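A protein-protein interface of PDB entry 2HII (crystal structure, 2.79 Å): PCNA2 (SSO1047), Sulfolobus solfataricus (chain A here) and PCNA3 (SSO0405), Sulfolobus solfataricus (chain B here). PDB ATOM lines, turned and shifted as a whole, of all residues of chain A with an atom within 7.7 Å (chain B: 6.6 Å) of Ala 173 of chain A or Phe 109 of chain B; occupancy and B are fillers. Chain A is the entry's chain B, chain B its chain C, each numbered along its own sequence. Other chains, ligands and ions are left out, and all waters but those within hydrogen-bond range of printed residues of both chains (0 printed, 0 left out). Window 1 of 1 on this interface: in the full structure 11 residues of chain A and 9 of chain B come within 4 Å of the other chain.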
ATOM      1  N   GLU A 145      -7.728  17.345  -7.616  1.00  0.00           N
ATOM      2  CA  GLU A 145      -7.232  18.677  -7.918  1.00  0.00           C
ATOM      3  C   GLU A 145      -5.720  18.683  -8.146  1.00  0.00           C
ATOM      4  O   GLU A 145      -5.232  19.456  -8.969  1.00  0.00           O
ATOM      5  CB  GLU A 145      -7.605  19.666  -6.804  1.00  0.00           C
ATOM      6  CG  GLU A 145      -9.130  19.891  -6.595  1.00  0.00           C
ATOM      7  CD  GLU A 145      -9.471  20.580  -5.249  1.00  0.00           C
ATOM      8  OE1 GLU A 145      -8.638  20.559  -4.310  1.00  0.00           O
ATOM      9  OE2 GLU A 145     -10.583  21.138  -5.120  1.00  0.00           O
ATOM     10  N   LEU A 146      -4.990  17.822  -7.440  1.00  0.00           N
ATOM     11  CA  LEU A 146      -3.526  17.847  -7.490  1.00  0.00           C
ATOM     12  C   LEU A 146      -2.906  16.969  -8.587  1.00  0.00           C
ATOM     13  O   LEU A 146      -1.975  17.399  -9.276  1.00  0.00           O
ATOM     14  CB  LEU A 146      -2.924  17.503  -6.122  1.00  0.00           C
ATOM     15  CG  LEU A 146      -3.059  18.471  -4.937  1.00  0.00           C
ATOM     16  CD1 LEU A 146      -2.207  17.995  -3.803  1.00  0.00           C
ATOM     17  CD2 LEU A 146      -2.658  19.884  -5.299  1.00  0.00           C
ATOM     18  N   LEU A 149      -1.084  18.157 -11.621  1.00  0.00           N
ATOM     19  CA  LEU A 149      -0.002  19.127 -11.492  1.00  0.00           C
ATOM     20  C   LEU A 149       1.375  18.482 -11.292  1.00  0.00           C
ATOM     21  O   LEU A 149       2.383  19.186 -11.165  1.00  0.00           O
ATOM     22  CB  LEU A 149      -0.308  20.112 -10.344  1.00  0.00           C
ATOM     23  CG  LEU A 149      -1.714  20.743 -10.219  1.00  0.00           C
ATOM     24  CD1 LEU A 149      -2.005  21.265  -8.809  1.00  0.00           C
ATOM     25  CD2 LEU A 149      -1.932  21.841 -11.246  1.00  0.00           C
ATOM     26  N   LEU A 153       3.676  13.322  -5.342  1.00  0.00           N
ATOM     27  CA  LEU A 153       2.986  13.953  -4.219  1.00  0.00           C
ATOM     28  C   LEU A 153       3.925  14.044  -3.027  1.00  0.00           C
ATOM     29  O   LEU A 153       4.425  13.032  -2.545  1.00  0.00           O
ATOM     30  CB  LEU A 153       1.764  13.123  -3.814  1.00  0.00           C
ATOM     31  CG  LEU A 153       0.616  13.689  -2.956  1.00  0.00           C
ATOM     32  CD1 LEU A 153       0.375  12.747  -1.776  1.00  0.00           C
ATOM     33  CD2 LEU A 153       0.814  15.134  -2.460  1.00  0.00           C
ATOM     34  N   ASN A 154       4.173  15.257  -2.553  1.00  0.00           N
ATOM     35  CA  ASN A 154       4.982  15.448  -1.355  1.00  0.00           C
ATOM     36  C   ASN A 154       4.083  15.680  -0.155  1.00  0.00           C
ATOM     37  O   ASN A 154       3.187  16.517  -0.197  1.00  0.00           O
ATOM     38  CB  ASN A 154       5.962  16.617  -1.535  1.00  0.00           C
ATOM     39  CG  ASN A 154       7.253  16.206  -2.227  1.00  0.00           C
ATOM     40  OD1 ASN A 154       8.067  15.487  -1.657  1.00  0.00           O
ATOM     41  ND2 ASN A 154       7.451  16.675  -3.455  1.00  0.00           N
ATOM     42  N   TYR A 163       0.263  18.579   5.405  1.00  0.00           N
ATOM     43  CA  TYR A 163       0.474  19.293   4.154  1.00  0.00           C
ATOM     44  C   TYR A 163       0.615  18.362   2.966  1.00  0.00           C
ATOM     45  O   TYR A 163       1.456  17.462   2.968  1.00  0.00           O
ATOM     46  CB  TYR A 163       1.719  20.176   4.255  1.00  0.00           C
ATOM     47  CG  TYR A 163       1.632  21.251   5.305  1.00  0.00           C
ATOM     48  CD1 TYR A 163       1.918  20.976   6.642  1.00  0.00           C
ATOM     49  CD2 TYR A 163       1.251  22.549   4.963  1.00  0.00           C
ATOM     50  CE1 TYR A 163       1.831  21.972   7.617  1.00  0.00           C
ATOM     51  CE2 TYR A 163       1.161  23.561   5.929  1.00  0.00           C
ATOM     52  CZ  TYR A 163       1.454  23.265   7.251  1.00  0.00           C
ATOM     53  OH  TYR A 163       1.365  24.255   8.201  1.00  0.00           O
ATOM     54  N   PHE A 164      -0.220  18.586   1.958  1.00  0.00           N
ATOM     55  CA  PHE A 164      -0.045  17.965   0.651  1.00  0.00           C
ATOM     56  C   PHE A 164       0.528  19.007  -0.290  1.00  0.00           C
ATOM     57  O   PHE A 164      -0.038  20.090  -0.442  1.00  0.00           O
ATOM     58  CB  PHE A 164      -1.372  17.476   0.084  1.00  0.00           C
ATOM     59  CG  PHE A 164      -1.906  16.257   0.744  1.00  0.00           C
ATOM     60  CD1 PHE A 164      -3.231  15.902   0.577  1.00  0.00           C
ATOM     61  CD2 PHE A 164      -1.105  15.457   1.527  1.00  0.00           C
ATOM     62  CE1 PHE A 164      -3.750  14.763   1.168  1.00  0.00           C
ATOM     63  CE2 PHE A 164      -1.621  14.323   2.133  1.00  0.00           C
ATOM     64  CZ  PHE A 164      -2.944  13.980   1.952  1.00  0.00           C
ATOM     65  N   GLU A 165       1.638  18.674  -0.933  1.00  0.00           N
ATOM     66  CA  GLU A 165       2.331  19.624  -1.779  1.00  0.00           C
ATOM     67  C   GLU A 165       2.717  19.014  -3.111  1.00  0.00           C
ATOM     68  O   GLU A 165       2.891  17.808  -3.207  1.00  0.00           O
ATOM     69  CB  GLU A 165       3.598  20.114  -1.080  1.00  0.00           C
ATOM     70  CG  GLU A 165       3.397  21.239  -0.087  1.00  0.00           C
ATOM     71  CD  GLU A 165       4.713  21.821   0.383  1.00  0.00           C
ATOM     72  OE1 GLU A 165       5.510  21.079   0.979  1.00  0.00           O
ATOM     73  OE2 GLU A 165       4.954  23.021   0.164  1.00  0.00           O
ATOM     74  N   VAL A 166       2.854  19.859  -4.130  1.00  0.00           N
ATOM     75  CA  VAL A 166       3.441  19.472  -5.414  1.00  0.00           C
ATOM     76  C   VAL A 166       4.508  20.490  -5.814  1.00  0.00           C
ATOM     77  O   VAL A 166       4.202  21.634  -6.146  1.00  0.00           O
ATOM     78  CB  VAL A 166       2.381  19.326  -6.520  1.00  0.00           C
ATOM     79  CG1 VAL A 166       3.036  19.236  -7.893  1.00  0.00           C
ATOM     80  CG2 VAL A 166       1.509  18.111  -6.263  1.00  0.00           C
ATOM     81  N   ILE A 167       5.762  20.054  -5.763  1.00  0.00           N
ATOM     82  CA  ILE A 167       6.916  20.907  -6.017  1.00  0.00           C
ATOM     83  C   ILE A 167       7.361  20.789  -7.468  1.00  0.00           C
ATOM     84  O   ILE A 167       7.529  19.692  -7.989  1.00  0.00           O
ATOM     85  CB  ILE A 167       8.074  20.561  -5.055  1.00  0.00           C
ATOM     86  CG1 ILE A 167       7.651  20.883  -3.613  1.00  0.00           C
ATOM     87  CG2 ILE A 167       9.358  21.315  -5.433  1.00  0.00           C
ATOM     88  CD1 ILE A 167       8.179  19.909  -2.558  1.00  0.00           C
ATOM     89  N   GLY A 168       7.512  21.937  -8.116  1.00  0.00           N
ATOM     90  CA  GLY A 168       8.034  22.013  -9.468  1.00  0.00           C
ATOM     91  C   GLY A 168       9.024  23.153  -9.495  1.00  0.00           C
ATOM     92  O   GLY A 168       9.017  24.014  -8.605  1.00  0.00           O
ATOM     93  N   SER A 171       6.564  26.269 -10.267  1.00  0.00           N
ATOM     94  CA  SER A 171       5.545  26.625  -9.290  1.00  0.00           C
ATOM     95  C   SER A 171       5.419  25.527  -8.251  1.00  0.00           C
ATOM     96  O   SER A 171       5.871  24.404  -8.468  1.00  0.00           O
ATOM     97  CB  SER A 171       4.192  26.797  -9.968  1.00  0.00           C
ATOM     98  OG  SER A 171       3.582  25.535 -10.184  1.00  0.00           O
ATOM     99  N   THR A 172       4.782  25.846  -7.131  1.00  0.00           N
ATOM    100  CA  THR A 172       4.439  24.828  -6.148  1.00  0.00           C
ATOM    101  C   THR A 172       3.016  24.956  -5.600  1.00  0.00           C
ATOM    102  O   THR A 172       2.586  26.031  -5.165  1.00  0.00           O
ATOM    103  CB  THR A 172       5.458  24.742  -4.990  1.00  0.00           C
ATOM    104  OG1 THR A 172       4.931  23.879  -3.973  1.00  0.00           O
ATOM    105  CG2 THR A 172       5.742  26.111  -4.388  1.00  0.00           C
ATOM    106  N   ALA A 173       2.301  23.836  -5.632  1.00  0.00           N
ATOM    107  CA  ALA A 173       0.967  23.720  -5.058  1.00  0.00           C
ATOM    108  C   ALA A 173       1.054  23.221  -3.620  1.00  0.00           C
ATOM    109  O   ALA A 173       1.901  22.394  -3.295  1.00  0.00           O
ATOM    110  CB  ALA A 173       0.127  22.788  -5.890  1.00  0.00           C
ATOM    111  N   LYS A 174       0.157  23.711  -2.771  1.00  0.00           N
ATOM    112  CA  LYS A 174       0.236  23.515  -1.319  1.00  0.00           C
ATOM    113  C   LYS A 174      -1.186  23.436  -0.735  1.00  0.00           C
ATOM    114  O   LYS A 174      -2.046  24.262  -1.069  1.00  0.00           O
ATOM    115  CB  LYS A 174       0.983  24.708  -0.710  1.00  0.00           C
ATOM    116  CG  LYS A 174       1.769  24.422   0.564  1.00  0.00           C
ATOM    117  CD  LYS A 174       2.473  25.707   1.032  1.00  0.00           C
ATOM    118  CE  LYS A 174       3.545  25.418   2.080  1.00  0.00           C
ATOM    119  NZ  LYS A 174       4.070  26.669   2.698  1.00  0.00           N
ATOM    120  N   VAL A 175      -1.446  22.437   0.106  1.00  0.00           N
ATOM    121  CA  VAL A 175      -2.737  22.342   0.809  1.00  0.00           C
ATOM    122  C   VAL A 175      -2.526  22.014   2.280  1.00  0.00           C
ATOM    123  O   VAL A 175      -1.954  20.982   2.620  1.00  0.00           O
ATOM    124  CB  VAL A 175      -3.697  21.281   0.212  1.00  0.00           C
ATOM    125  CG1 VAL A 175      -5.062  21.402   0.864  1.00  0.00           C
ATOM    126  CG2 VAL A 175      -3.835  21.442  -1.287  1.00  0.00           C
ATOM    127  N   TYR B  73      -0.864  27.170 -18.132  1.00  0.00           N
ATOM    128  CA  TYR B  73      -0.682  26.829 -16.732  1.00  0.00           C
ATOM    129  C   TYR B  73      -1.678  27.528 -15.830  1.00  0.00           C
ATOM    130  O   TYR B  73      -2.312  26.897 -15.005  1.00  0.00           O
ATOM    131  CB  TYR B  73       0.723  27.159 -16.262  1.00  0.00           C
ATOM    132  CG  TYR B  73       0.876  26.925 -14.786  1.00  0.00           C
ATOM    133  CD1 TYR B  73       0.930  25.628 -14.281  1.00  0.00           C
ATOM    134  CD2 TYR B  73       0.935  27.991 -13.894  1.00  0.00           C
ATOM    135  CE1 TYR B  73       1.055  25.389 -12.935  1.00  0.00           C
ATOM    136  CE2 TYR B  73       1.056  27.763 -12.533  1.00  0.00           C
ATOM    137  CZ  TYR B  73       1.118  26.454 -12.061  1.00  0.00           C
ATOM    138  OH  TYR B  73       1.245  26.190 -10.715  1.00  0.00           O
ATOM    139  N   LYS B  76      -4.881  25.662 -15.900  1.00  0.00           N
ATOM    140  CA  LYS B  76      -4.975  24.580 -14.937  1.00  0.00           C
ATOM    141  C   LYS B  76      -5.461  25.065 -13.575  1.00  0.00           C
ATOM    142  O   LYS B  76      -6.439  24.546 -13.046  1.00  0.00           O
ATOM    143  CB  LYS B  76      -3.646  23.822 -14.817  1.00  0.00           C
ATOM    144  CG  LYS B  76      -3.607  22.584 -15.690  1.00  0.00           C
ATOM    145  CD  LYS B  76      -2.218  22.028 -15.880  1.00  0.00           C
ATOM    146  CE  LYS B  76      -2.231  21.054 -17.040  1.00  0.00           C
ATOM    147  NZ  LYS B  76      -1.230  19.978 -16.847  1.00  0.00           N
ATOM    148  N   ILE B  77      -4.813  26.079 -13.019  1.00  0.00           N
ATOM    149  CA  ILE B  77      -5.076  26.411 -11.633  1.00  0.00           C
ATOM    150  C   ILE B  77      -6.479  26.998 -11.501  1.00  0.00           C
ATOM    151  O   ILE B  77      -7.135  26.800 -10.484  1.00  0.00           O
ATOM    152  CB  ILE B  77      -3.950  27.289 -10.974  1.00  0.00           C
ATOM    153  CG1 ILE B  77      -4.348  28.745 -10.854  1.00  0.00           C
ATOM    154  CG2 ILE B  77      -2.626  27.175 -11.725  1.00  0.00           C
ATOM    155  CD1 ILE B  77      -3.266  29.594 -10.259  1.00  0.00           C
ATOM    156  N   LEU B  78      -6.953  27.676 -12.542  1.00  0.00           N
ATOM    157  CA  LEU B  78      -8.279  28.275 -12.510  1.00  0.00           C
ATOM    158  C   LEU B  78      -9.381  27.228 -12.661  1.00  0.00           C
ATOM    159  O   LEU B  78     -10.492  27.391 -12.155  1.00  0.00           O
ATOM    160  CB  LEU B  78      -8.396  29.348 -13.584  1.00  0.00           C
ATOM    161  CG  LEU B  78      -7.448  30.539 -13.456  1.00  0.00           C
ATOM    162  CD1 LEU B  78      -7.684  31.467 -14.617  1.00  0.00           C
ATOM    163  CD2 LEU B  78      -7.650  31.260 -12.154  1.00  0.00           C
ATOM    164  N   VAL B  80      -9.388  24.423 -11.196  1.00  0.00           N
ATOM    165  CA  VAL B  80      -9.544  23.644  -9.937  1.00  0.00           C
ATOM    166  C   VAL B  80     -10.923  23.878  -9.324  1.00  0.00           C
ATOM    167  O   VAL B  80     -11.513  22.965  -8.742  1.00  0.00           O
ATOM    168  CB  VAL B  80      -8.422  23.862  -8.823  1.00  0.00           C
ATOM    169  CG1 VAL B  80      -6.998  23.795  -9.387  1.00  0.00           C
ATOM    170  CG2 VAL B  80      -8.653  25.108  -7.985  1.00  0.00           C
ATOM    171  N   VAL B  97       4.506  35.207  -7.571  1.00  0.00           N
ATOM    172  CA  VAL B  97       3.077  35.460  -7.406  1.00  0.00           C
ATOM    173  C   VAL B  97       2.456  34.329  -6.587  1.00  0.00           C
ATOM    174  O   VAL B  97       2.699  33.152  -6.873  1.00  0.00           O
ATOM    175  CB  VAL B  97       2.344  35.673  -8.780  1.00  0.00           C
ATOM    176  CG1 VAL B  97       0.850  35.785  -8.594  1.00  0.00           C
ATOM    177  CG2 VAL B  97       2.856  36.932  -9.471  1.00  0.00           C
ATOM    178  N   ILE B  98       1.682  34.691  -5.558  1.00  0.00           N
ATOM    179  CA  ILE B  98       1.019  33.689  -4.730  1.00  0.00           C
ATOM    180  C   ILE B  98      -0.471  33.739  -4.971  1.00  0.00           C
ATOM    181  O   ILE B  98      -1.123  34.754  -4.689  1.00  0.00           O
ATOM    182  CB  ILE B  98       1.341  33.814  -3.208  1.00  0.00           C
ATOM    183  CG1 ILE B  98       2.853  33.670  -2.951  1.00  0.00           C
ATOM    184  CG2 ILE B  98       0.580  32.739  -2.425  1.00  0.00           C
ATOM    185  CD1 ILE B  98       3.278  33.601  -1.478  1.00  0.00           C
ATOM    186  N   ILE B  99      -0.998  32.631  -5.489  1.00  0.00           N
ATOM    187  CA  ILE B  99      -2.413  32.522  -5.810  1.00  0.00           C
ATOM    188  C   ILE B  99      -3.133  31.573  -4.860  1.00  0.00           C
ATOM    189  O   ILE B  99      -2.733  30.416  -4.722  1.00  0.00           O
ATOM    190  CB  ILE B  99      -2.622  32.086  -7.266  1.00  0.00           C
ATOM    191  CG1 ILE B  99      -2.022  33.126  -8.213  1.00  0.00           C
ATOM    192  CG2 ILE B  99      -4.108  31.880  -7.550  1.00  0.00           C
ATOM    193  CD1 ILE B  99      -1.855  32.655  -9.647  1.00  0.00           C
ATOM    194  N   ASN B 100      -4.181  32.075  -4.206  1.00  0.00           N
ATOM    195  CA  ASN B 100      -5.046  31.265  -3.351  1.00  0.00           C
ATOM    196  C   ASN B 100      -6.458  31.105  -3.914  1.00  0.00           C
ATOM    197  O   ASN B 100      -7.142  32.091  -4.204  1.00  0.00           O
ATOM    198  CB  ASN B 100      -5.143  31.864  -1.958  1.00  0.00           C
ATOM    199  CG  ASN B 100      -4.044  31.393  -1.044  1.00  0.00           C
ATOM    200  OD1 ASN B 100      -4.306  30.705  -0.053  1.00  0.00           O
ATOM    201  ND2 ASN B 100      -2.801  31.766  -1.358  1.00  0.00           N
ATOM    202  N   ILE B 101      -6.887  29.855  -4.068  1.00  0.00           N
ATOM    203  CA  ILE B 101      -8.227  29.550  -4.558  1.00  0.00           C
ATOM    204  C   ILE B 101      -8.962  28.974  -3.364  1.00  0.00           C
ATOM    205  O   ILE B 101      -8.584  27.899  -2.872  1.00  0.00           O
ATOM    206  CB  ILE B 101      -8.219  28.511  -5.720  1.00  0.00           C
ATOM    207  CG1 ILE B 101      -7.153  28.831  -6.786  1.00  0.00           C
ATOM    208  CG2 ILE B 101      -9.601  28.391  -6.345  1.00  0.00           C
ATOM    209  CD1 ILE B 101      -7.572  29.765  -7.883  1.00  0.00           C
ATOM    210  N   ARG B 107      -6.437  26.046  -1.721  1.00  0.00           N
ATOM    211  CA  ARG B 107      -5.353  25.628  -2.622  1.00  0.00           C
ATOM    212  C   ARG B 107      -4.387  26.774  -2.938  1.00  0.00           C
ATOM    213  O   ARG B 107      -4.735  27.695  -3.689  1.00  0.00           O
ATOM    214  CB  ARG B 107      -5.940  25.153  -3.960  1.00  0.00           C
ATOM    215  CG  ARG B 107      -6.634  23.802  -3.983  1.00  0.00           C
ATOM    216  CD  ARG B 107      -7.777  23.701  -2.985  1.00  0.00           C
ATOM    217  NE  ARG B 107      -8.791  24.748  -3.113  1.00  0.00           N
ATOM    218  CZ  ARG B 107      -9.762  24.749  -4.023  1.00  0.00           C
ATOM    219  NH1 ARG B 107      -9.840  23.774  -4.919  1.00  0.00           N
ATOM    220  NH2 ARG B 107     -10.657  25.732  -4.050  1.00  0.00           N
ATOM    221  N   GLU B 108      -3.172  26.705  -2.400  1.00  0.00           N
ATOM    222  CA  GLU B 108      -2.176  27.759  -2.600  1.00  0.00           C
ATOM    223  C   GLU B 108      -1.241  27.407  -3.747  1.00  0.00           C
ATOM    224  O   GLU B 108      -0.813  26.268  -3.847  1.00  0.00           O
ATOM    225  CB  GLU B 108      -1.380  27.956  -1.309  1.00  0.00           C
ATOM    226  CG  GLU B 108      -0.036  28.636  -1.494  1.00  0.00           C
ATOM    227  CD  GLU B 108       0.481  29.230  -0.214  1.00  0.00           C
ATOM    228  OE1 GLU B 108      -0.288  29.989   0.421  1.00  0.00           O
ATOM    229  OE2 GLU B 108       1.645  28.941   0.156  1.00  0.00           O
ATOM    230  N   PHE B 109      -0.926  28.369  -4.610  1.00  0.00           N
ATOM    231  CA  PHE B 109       0.081  28.136  -5.651  1.00  0.00           C
ATOM    232  C   PHE B 109       1.122  29.223  -5.574  1.00  0.00           C
ATOM    233  O   PHE B 109       0.816  30.402  -5.760  1.00  0.00           O
ATOM    234  CB  PHE B 109      -0.522  28.109  -7.063  1.00  0.00           C
ATOM    235  CG  PHE B 109      -1.554  27.038  -7.269  1.00  0.00           C
ATOM    236  CD1 PHE B 109      -2.838  27.160  -6.725  1.00  0.00           C
ATOM    237  CD2 PHE B 109      -1.260  25.913  -8.022  1.00  0.00           C
ATOM    238  CE1 PHE B 109      -3.803  26.167  -6.914  1.00  0.00           C
ATOM    239  CE2 PHE B 109      -2.228  24.917  -8.227  1.00  0.00           C
ATOM    240  CZ  PHE B 109      -3.498  25.047  -7.667  1.00  0.00           C
ATOM    241  N   ASN B 110       2.350  28.826  -5.270  1.00  0.00           N
ATOM    242  CA  ASN B 110       3.463  29.750  -5.289  1.00  0.00           C
ATOM    243  C   ASN B 110       4.086  29.716  -6.679  1.00  0.00           C
ATOM    244  O   ASN B 110       4.846  28.802  -7.003  1.00  0.00           O
ATOM    245  CB  ASN B 110       4.486  29.359  -4.233  1.00  0.00           C
ATOM    246  CG  ASN B 110       5.491  30.449  -3.964  1.00  0.00           C
ATOM    247  OD1 ASN B 110       6.220  30.889  -4.857  1.00  0.00           O
ATOM    248  ND2 ASN B 110       5.545  30.892  -2.716  1.00  0.00           N
ATOM    249  N   VAL B 111       3.745  30.698  -7.511  1.00  0.00           N
ATOM    250  CA  VAL B 111       4.213  30.703  -8.884  1.00  0.00           C
ATOM    251  C   VAL B 111       5.393  31.639  -9.049  1.00  0.00           C
ATOM    252  O   VAL B 111       5.403  32.757  -8.526  1.00  0.00           O
ATOM    253  CB  VAL B 111       3.091  31.065  -9.879  1.00  0.00           C
ATOM    254  CG1 VAL B 111       3.576  30.934 -11.327  1.00  0.00           C
ATOM    255  CG2 VAL B 111       1.875  30.173  -9.662  1.00  0.00           C
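Of the printed residues of chain B, Leu 149 of chain A touches Phe 109 (3.7 Å).
Printed residues of chain B within 4 Å of Ser 171 of chain A: Tyr 73 and Asn 110.
Printed residues of chain B within 4 Å of Thr 172 of chain A: Glu 108, Phe 109 and Asn 110.
Ala 173 of chain A touches just these residues of chain B: Glu 108 and Phe 109.
Of the printed residues of chain B, Lys 174 of chain A touches Arg 107 and Glu 108.
Of the printed residues of chain A, Glu 108 of chain B touches Thr 172 (3.7 Å), Ala 173 (3.3 Å) and Lys 174 (2.9 Å).
Phe 109 of chain B touches three residues of chain A.
The nearest residue of chain B that does not touch Ala 173 of chain A is Asn 110 of chain B (5.0 Å).
The backbone carbonyl oxygen of Val 166 of chain A lies close to the side-chain hydroxyl of Thr 172 of chain A.
The backbone NH of Val 166 of chain A lies within hydrogen-bond range of the backbone carbonyl oxygen of Ala 173 of chain A (2.8 Å).
The backbone carbonyl oxygen of Ile 99 of chain B lies within hydrogen-bond range of the backbone NH of Phe 109 of chain B (2.7 Å).
O of Ile 101 of chain B sits at hydrogen-bond distance from N of Arg 107 of chain B.
The side-chain carboxylate (OE2) of Glu 145 of chain A lies within salt-bridge range of the guanidinium group (NH1) of Arg 107 of chain B (2.7 Å).
The side-chain hydroxyl of Ser 171 of chain A sits at hydrogen-bond distance from the side-chain hydroxyl of Tyr 73 of chain B.
N of Asn 110 of chain B sits at hydrogen-bond distance from O of Thr 172 of chain A (2.8 Å).
The backbone carbonyl oxygen (O) of Glu 108 of chain B sits at hydrogen-bond distance from the backbone NH (N) of Lys 174 of chain A (2.9 Å).
CE2 of Phe 109 of chain B touches CD1 of Leu 149 of chain A, at 3.7 Å.
Asn 110 of chain B touches Ser 171 of chain A.
Thr 172 of chain A touches Glu 108 of chain B (O to O, 3.7 Å).
Thr 172 of chain A touches Phe 109 of chain B (O to CA, 3.3 Å).
Ala 173 of chain A touches Glu 108 of chain B.
Phe 109 of chain B touches Ala 173 of chain A (CE2 to CB, 3.9 Å).
O of Lys 174 of chain A touches CA of Arg 107 of chain B, 3.9 Å away.
Of the 15 printed residues of chain B, 5 touch a printed residue of chain A.
Printed residues of chain B that touch a printed residue of chain A: Tyr 73, Arg 107, Glu 108, Phe 109 and Asn 110.
Hydrophobic or aromatic side chains of chain B within 4 Å of the printed part of chain A: Tyr 73 and Phe 109.
Along chain A the printed residues that touch a printed residue of chain B span positions 145 to 174.
Among the printed residues, 11 pairs touch across the chains.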
